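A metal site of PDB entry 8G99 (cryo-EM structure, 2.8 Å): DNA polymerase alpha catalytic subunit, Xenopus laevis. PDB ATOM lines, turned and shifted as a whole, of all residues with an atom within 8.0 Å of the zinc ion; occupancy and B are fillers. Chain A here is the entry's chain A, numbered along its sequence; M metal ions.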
ATOM      1  N   PHE A 947       6.593  -0.440  23.244  1.00  0.00           N
ATOM      2  CA  PHE A 947       7.723  -0.846  22.422  1.00  0.00           C
ATOM      3  C   PHE A 947       7.642  -0.163  21.067  1.00  0.00           C
ATOM      4  O   PHE A 947       6.626  -0.262  20.383  1.00  0.00           O
ATOM      5  CB  PHE A 947       7.761  -2.368  22.249  1.00  0.00           C
ATOM      6  CG  PHE A 947       8.956  -2.862  21.488  1.00  0.00           C
ATOM      7  CD1 PHE A 947      10.225  -2.609  21.948  1.00  0.00           C
ATOM      8  CD2 PHE A 947       8.797  -3.577  20.322  1.00  0.00           C
ATOM      9  CE1 PHE A 947      11.329  -3.062  21.251  1.00  0.00           C
ATOM     10  CE2 PHE A 947       9.893  -4.037  19.625  1.00  0.00           C
ATOM     11  CZ  PHE A 947      11.156  -3.775  20.085  1.00  0.00           C
ATOM     12  N   PHE A 948       8.708   0.531  20.693  1.00  0.00           N
ATOM     13  CA  PHE A 948       8.754   1.227  19.410  1.00  0.00           C
ATOM     14  C   PHE A 948       9.268   0.289  18.333  1.00  0.00           C
ATOM     15  O   PHE A 948      10.333  -0.325  18.480  1.00  0.00           O
ATOM     16  CB  PHE A 948       9.644   2.463  19.510  1.00  0.00           C
ATOM     17  CG  PHE A 948       9.016   3.605  20.231  1.00  0.00           C
ATOM     18  CD1 PHE A 948       7.934   4.268  19.692  1.00  0.00           C
ATOM     19  CD2 PHE A 948       9.505   4.021  21.463  1.00  0.00           C
ATOM     20  CE1 PHE A 948       7.345   5.325  20.365  1.00  0.00           C
ATOM     21  CE2 PHE A 948       8.921   5.070  22.127  1.00  0.00           C
ATOM     22  CZ  PHE A 948       7.845   5.725  21.577  1.00  0.00           C
ATOM     23  N   CYS A 949       8.504   0.177  17.243  1.00  0.00           N
ATOM     24  CA  CYS A 949       8.903  -0.700  16.161  1.00  0.00           C
ATOM     25  C   CYS A 949      10.233  -0.243  15.582  1.00  0.00           C
ATOM     26  O   CYS A 949      10.381   0.940  15.240  1.00  0.00           O
ATOM     27  CB  CYS A 949       7.830  -0.704  15.064  1.00  0.00           C
ATOM     28  SG  CYS A 949       7.968  -2.067  13.883  1.00  0.00           S
ATOM     29  N   PRO A 950      11.227  -1.122  15.456  1.00  0.00           N
ATOM     30  CA  PRO A 950      12.487  -0.695  14.844  1.00  0.00           C
ATOM     31  C   PRO A 950      12.326  -0.209  13.413  1.00  0.00           C
ATOM     32  O   PRO A 950      13.060   0.692  12.989  1.00  0.00           O
ATOM     33  CB  PRO A 950      13.361  -1.957  14.906  1.00  0.00           C
ATOM     34  CG  PRO A 950      12.686  -2.860  15.868  1.00  0.00           C
ATOM     35  CD  PRO A 950      11.247  -2.554  15.811  1.00  0.00           C
ATOM     36  N   LYS A 951      11.379  -0.780  12.670  1.00  0.00           N
ATOM     37  CA  LYS A 951      11.240  -0.444  11.256  1.00  0.00           C
ATOM     38  C   LYS A 951      10.491   0.869  11.063  1.00  0.00           C
ATOM     39  O   LYS A 951      11.033   1.831  10.517  1.00  0.00           O
ATOM     40  CB  LYS A 951      10.529  -1.586  10.517  1.00  0.00           C
ATOM     41  CG  LYS A 951      10.629  -1.506   9.012  1.00  0.00           C
ATOM     42  CD  LYS A 951      10.123  -2.777   8.348  1.00  0.00           C
ATOM     43  CE  LYS A 951      10.141  -2.661   6.836  1.00  0.00           C
ATOM     44  NZ  LYS A 951       9.577  -3.876   6.182  1.00  0.00           N
ATOM     45  N   CYS A 952       9.234   0.924  11.520  1.00  0.00           N
ATOM     46  CA  CYS A 952       8.407   2.095  11.309  1.00  0.00           C
ATOM     47  C   CYS A 952       8.501   3.119  12.423  1.00  0.00           C
ATOM     48  O   CYS A 952       8.207   4.301  12.199  1.00  0.00           O
ATOM     49  CB  CYS A 952       6.940   1.692  11.130  1.00  0.00           C
ATOM     50  SG  CYS A 952       6.181   0.954  12.591  1.00  0.00           S
ATOM     51  N   GLY A 953       8.913   2.708  13.623  1.00  0.00           N
ATOM     52  CA  GLY A 953       9.039   3.629  14.731  1.00  0.00           C
ATOM     53  C   GLY A 953       7.739   3.973  15.425  1.00  0.00           C
ATOM     54  O   GLY A 953       7.730   4.911  16.240  1.00  0.00           O
ATOM     55  N   THR A 954       6.650   3.271  15.139  1.00  0.00           N
ATOM     56  CA  THR A 954       5.383   3.538  15.796  1.00  0.00           C
ATOM     57  C   THR A 954       5.315   2.811  17.123  1.00  0.00           C
ATOM     58  O   THR A 954       5.771   1.672  17.254  1.00  0.00           O
ATOM     59  CB  THR A 954       4.216   3.121  14.907  1.00  0.00           C
ATOM     60  OG1 THR A 954       3.026   3.814  15.306  1.00  0.00           O
ATOM     61  CG2 THR A 954       3.965   1.621  15.002  1.00  0.00           C
ATOM     62  N   GLU A 955       4.741   3.480  18.126  1.00  0.00           N
ATOM     63  CA  GLU A 955       4.608   2.880  19.450  1.00  0.00           C
ATOM     64  C   GLU A 955       3.603   1.744  19.422  1.00  0.00           C
ATOM     65  O   GLU A 955       2.538   1.839  18.801  1.00  0.00           O
ATOM     66  CB  GLU A 955       4.172   3.935  20.456  1.00  0.00           C
ATOM     67  CG  GLU A 955       4.505   3.589  21.898  1.00  0.00           C
ATOM     68  CD  GLU A 955       4.542   4.812  22.794  1.00  0.00           C
ATOM     69  OE1 GLU A 955       3.536   5.538  22.849  1.00  0.00           O
ATOM     70  OE2 GLU A 955       5.591   5.040  23.429  1.00  0.00           O
ATOM     71  N   ASN A 956       3.934   0.658  20.121  1.00  0.00           N
ATOM     72  CA  ASN A 956       3.044  -0.462  20.326  1.00  0.00           C
ATOM     73  C   ASN A 956       2.769  -0.569  21.813  1.00  0.00           C
ATOM     74  O   ASN A 956       3.714  -0.684  22.613  1.00  0.00           O
ATOM     75  CB  ASN A 956       3.653  -1.761  19.794  1.00  0.00           C
ATOM     76  CG  ASN A 956       3.988  -1.694  18.325  1.00  0.00           C
ATOM     77  OD1 ASN A 956       3.196  -2.087  17.482  1.00  0.00           O
ATOM     78  ND2 ASN A 956       5.179  -1.208  18.015  1.00  0.00           N
ATOM     79  N   ARG A 975       2.420  -9.032  15.126  1.00  0.00           N
ATOM     80  CA  ARG A 975       2.267  -8.033  14.070  1.00  0.00           C
ATOM     81  C   ARG A 975       2.312  -6.636  14.666  1.00  0.00           C
ATOM     82  O   ARG A 975       1.880  -6.407  15.795  1.00  0.00           O
ATOM     83  CB  ARG A 975       0.959  -8.229  13.309  1.00  0.00           C
ATOM     84  CG  ARG A 975       0.807  -9.623  12.700  1.00  0.00           C
ATOM     85  CD  ARG A 975      -0.215  -9.662  11.571  1.00  0.00           C
ATOM     86  NE  ARG A 975      -1.588  -9.651  12.068  1.00  0.00           N
ATOM     87  CZ  ARG A 975      -2.298  -8.551  12.295  1.00  0.00           C
ATOM     88  NH1 ARG A 975      -1.798  -7.338  12.079  1.00  0.00           N
ATOM     89  NH2 ARG A 975      -3.544  -8.668  12.750  1.00  0.00           N
ATOM     90  N   CYS A 976       2.852  -5.702  13.891  1.00  0.00           N
ATOM     91  CA  CYS A 976       2.943  -4.319  14.314  1.00  0.00           C
ATOM     92  C   CYS A 976       1.564  -3.666  14.326  1.00  0.00           C
ATOM     93  O   CYS A 976       0.641  -4.089  13.613  1.00  0.00           O
ATOM     94  CB  CYS A 976       3.887  -3.531  13.401  1.00  0.00           C
ATOM     95  SG  CYS A 976       4.221  -1.846  13.934  1.00  0.00           S
ATOM     96  N   SER A 977       1.415  -2.622  15.143  1.00  0.00           N
ATOM     97  CA  SER A 977       0.146  -1.918  15.235  1.00  0.00           C
ATOM     98  C   SER A 977      -0.150  -1.102  13.987  1.00  0.00           C
ATOM     99  O   SER A 977      -1.301  -0.689  13.806  1.00  0.00           O
ATOM    100  CB  SER A 977       0.150  -1.007  16.461  1.00  0.00           C
ATOM    101  OG  SER A 977       0.624  -1.690  17.611  1.00  0.00           O
ATOM    102  N   LYS A 978       0.844  -0.856  13.139  1.00  0.00           N
ATOM    103  CA  LYS A 978       0.639  -0.068  11.927  1.00  0.00           C
ATOM    104  C   LYS A 978       0.296  -0.999  10.773  1.00  0.00           C
ATOM    105  O   LYS A 978       1.130  -1.841  10.404  1.00  0.00           O
ATOM    106  CB  LYS A 978       1.882   0.733  11.596  1.00  0.00           C
ATOM    107  CG  LYS A 978       1.720   1.698  10.442  1.00  0.00           C
ATOM    108  CD  LYS A 978       2.979   2.526  10.240  1.00  0.00           C
ATOM    109  CE  LYS A 978       2.857   3.472   9.064  1.00  0.00           C
ATOM    110  NZ  LYS A 978       4.079   4.282   8.855  1.00  0.00           N
ATOM    111  N   PRO A 979      -0.895  -0.891  10.169  1.00  0.00           N
ATOM    112  CA  PRO A 979      -1.228  -1.813   9.064  1.00  0.00           C
ATOM    113  C   PRO A 979      -0.236  -1.776   7.927  1.00  0.00           C
ATOM    114  O   PRO A 979       0.083  -2.822   7.350  1.00  0.00           O
ATOM    115  CB  PRO A 979      -2.622  -1.341   8.635  1.00  0.00           C
ATOM    116  CG  PRO A 979      -3.191  -0.669   9.829  1.00  0.00           C
ATOM    117  CD  PRO A 979      -2.035  -0.041  10.537  1.00  0.00           C
ATOM    118  N   GLU A 980       0.275  -0.593   7.582  1.00  0.00           N
ATOM    119  CA  GLU A 980       1.263  -0.495   6.512  1.00  0.00           C
ATOM    120  C   GLU A 980       2.603  -1.114   6.883  1.00  0.00           C
ATOM    121  O   GLU A 980       3.429  -1.317   5.989  1.00  0.00           O
ATOM    122  CB  GLU A 980       1.458   0.972   6.122  1.00  0.00           C
ATOM    123  CG  GLU A 980       0.337   1.551   5.299  1.00  0.00           C
ATOM    124  CD  GLU A 980       0.634   2.960   4.805  1.00  0.00           C
ATOM    125  OE1 GLU A 980       1.618   3.562   5.284  1.00  0.00           O
ATOM    126  OE2 GLU A 980      -0.119   3.466   3.942  1.00  0.00           O
ATOM    127  N   CYS A 981       2.839  -1.411   8.158  1.00  0.00           N
ATOM    128  CA  CYS A 981       4.098  -1.967   8.620  1.00  0.00           C
ATOM    129  C   CYS A 981       3.978  -3.490   8.678  1.00  0.00           C
ATOM    130  O   CYS A 981       3.066  -4.018   9.334  1.00  0.00           O
ATOM    131  CB  CYS A 981       4.487  -1.413   9.982  1.00  0.00           C
ATOM    132  SG  CYS A 981       6.006  -2.131  10.657  1.00  0.00           S
ATOM    133  N   ASP A 982       4.880  -4.186   7.996  1.00  0.00           N
ATOM    134  CA  ASP A 982       4.921  -5.641   8.000  1.00  0.00           C
ATOM    135  C   ASP A 982       5.884  -6.207   9.033  1.00  0.00           C
ATOM    136  O   ASP A 982       5.990  -7.427   9.151  1.00  0.00           O
ATOM    137  CB  ASP A 982       5.302  -6.158   6.609  1.00  0.00           C
ATOM    138  CG  ASP A 982       6.696  -5.725   6.198  1.00  0.00           C
ATOM    139  OD1 ASP A 982       7.230  -4.780   6.807  1.00  0.00           O
ATOM    140  OD2 ASP A 982       7.258  -6.339   5.272  1.00  0.00           O
ATOM    141  N   ALA A 983       6.574  -5.354   9.778  1.00  0.00           N
ATOM    142  CA  ALA A 983       7.563  -5.835  10.735  1.00  0.00           C
ATOM    143  C   ALA A 983       6.878  -6.577  11.880  1.00  0.00           C
ATOM    144  O   ALA A 983       5.848  -6.141  12.403  1.00  0.00           O
ATOM    145  CB  ALA A 983       8.379  -4.671  11.285  1.00  0.00           C
ATOM    146  N   SER A 984       7.463  -7.714  12.265  1.00  0.00           N
ATOM    147  CA  SER A 984       6.965  -8.497  13.380  1.00  0.00           C
ATOM    148  C   SER A 984       7.830  -8.224  14.596  1.00  0.00           C
ATOM    149  O   SER A 984       9.037  -8.513  14.557  1.00  0.00           O
ATOM    150  CB  SER A 984       6.976  -9.976  13.046  1.00  0.00           C
ATOM    151  OG  SER A 984       6.921 -10.771  14.215  1.00  0.00           O
ATOM    152  N   PRO A 985       7.291  -7.695  15.696  1.00  0.00           N
ATOM    153  CA  PRO A 985       8.127  -7.485  16.887  1.00  0.00           C
ATOM    154  C   PRO A 985       8.755  -8.768  17.407  1.00  0.00           C
ATOM    155  O   PRO A 985       9.803  -8.695  18.060  1.00  0.00           O
ATOM    156  CB  PRO A 985       7.148  -6.890  17.910  1.00  0.00           C
ATOM    157  CG  PRO A 985       6.081  -6.280  17.091  1.00  0.00           C
ATOM    158  CD  PRO A 985       5.939  -7.149  15.882  1.00  0.00           C
ATOM    159  N   TYR A 988      12.424  -8.990  16.608  1.00  0.00           N
ATOM    160  CA  TYR A 988      13.338  -8.224  17.454  1.00  0.00           C
ATOM    161  C   TYR A 988      13.046  -8.501  18.931  1.00  0.00           C
ATOM    162  O   TYR A 988      12.761  -7.595  19.714  1.00  0.00           O
ATOM    163  CB  TYR A 988      13.227  -6.737  17.142  1.00  0.00           C
ATOM    164  CG  TYR A 988      13.038  -6.428  15.673  1.00  0.00           C
ATOM    165  CD1 TYR A 988      11.783  -6.412  15.098  1.00  0.00           C
ATOM    166  CD2 TYR A 988      14.138  -6.147  14.867  1.00  0.00           C
ATOM    167  CE1 TYR A 988      11.614  -6.126  13.759  1.00  0.00           C
ATOM    168  CE2 TYR A 988      13.969  -5.860  13.528  1.00  0.00           C
ATOM    169  CZ  TYR A 988      12.707  -5.850  12.974  1.00  0.00           C
ATOM    170  OH  TYR A 988      12.539  -5.563  11.645  1.00  0.00           O
HETATM  171 ZN    ZN M   1       6.095  -1.291  12.755  1.00  0.00          ZN
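The backbone NH (N) of Lys 978 sits close to the side-chain sulfur (SG) of Cys 976. N of Cys 976 lies within hydrogen-bond range of O of Ala 983, 3.4 Å away. The side-chain sulfur of Cys 952 sits close to the backbone NH of Thr 954 (3.5 Å). The side-chain sulfur (SG) of Cys 976 sits close to the side-chain amide oxygen (OD1) of Asn 956, at 3.7 Å. N of Cys 949 sits at hydrogen-bond distance from O of Thr 954, 3.1 Å away. The backbone NH (N) of Ala 983 lies close to the side-chain sulfur (SG) of Cys 981, at 3.4 Å.
Of the 22 residues printed, 4 come within 4 Å of the zinc ion. The nearest printed residue that does not touch the zinc ion is Thr 954 (4.3 Å).
The zinc ion is bound by the side-chain sulfur of Cys 952 (2.3 Å), the side-chain sulfur of Cys 981 (2.3 Å), the side-chain sulfur of Cys 976 (2.3 Å) and the side-chain sulfur of Cys 949 (2.3 Å). The zinc ion has four donor atoms within binding distance.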
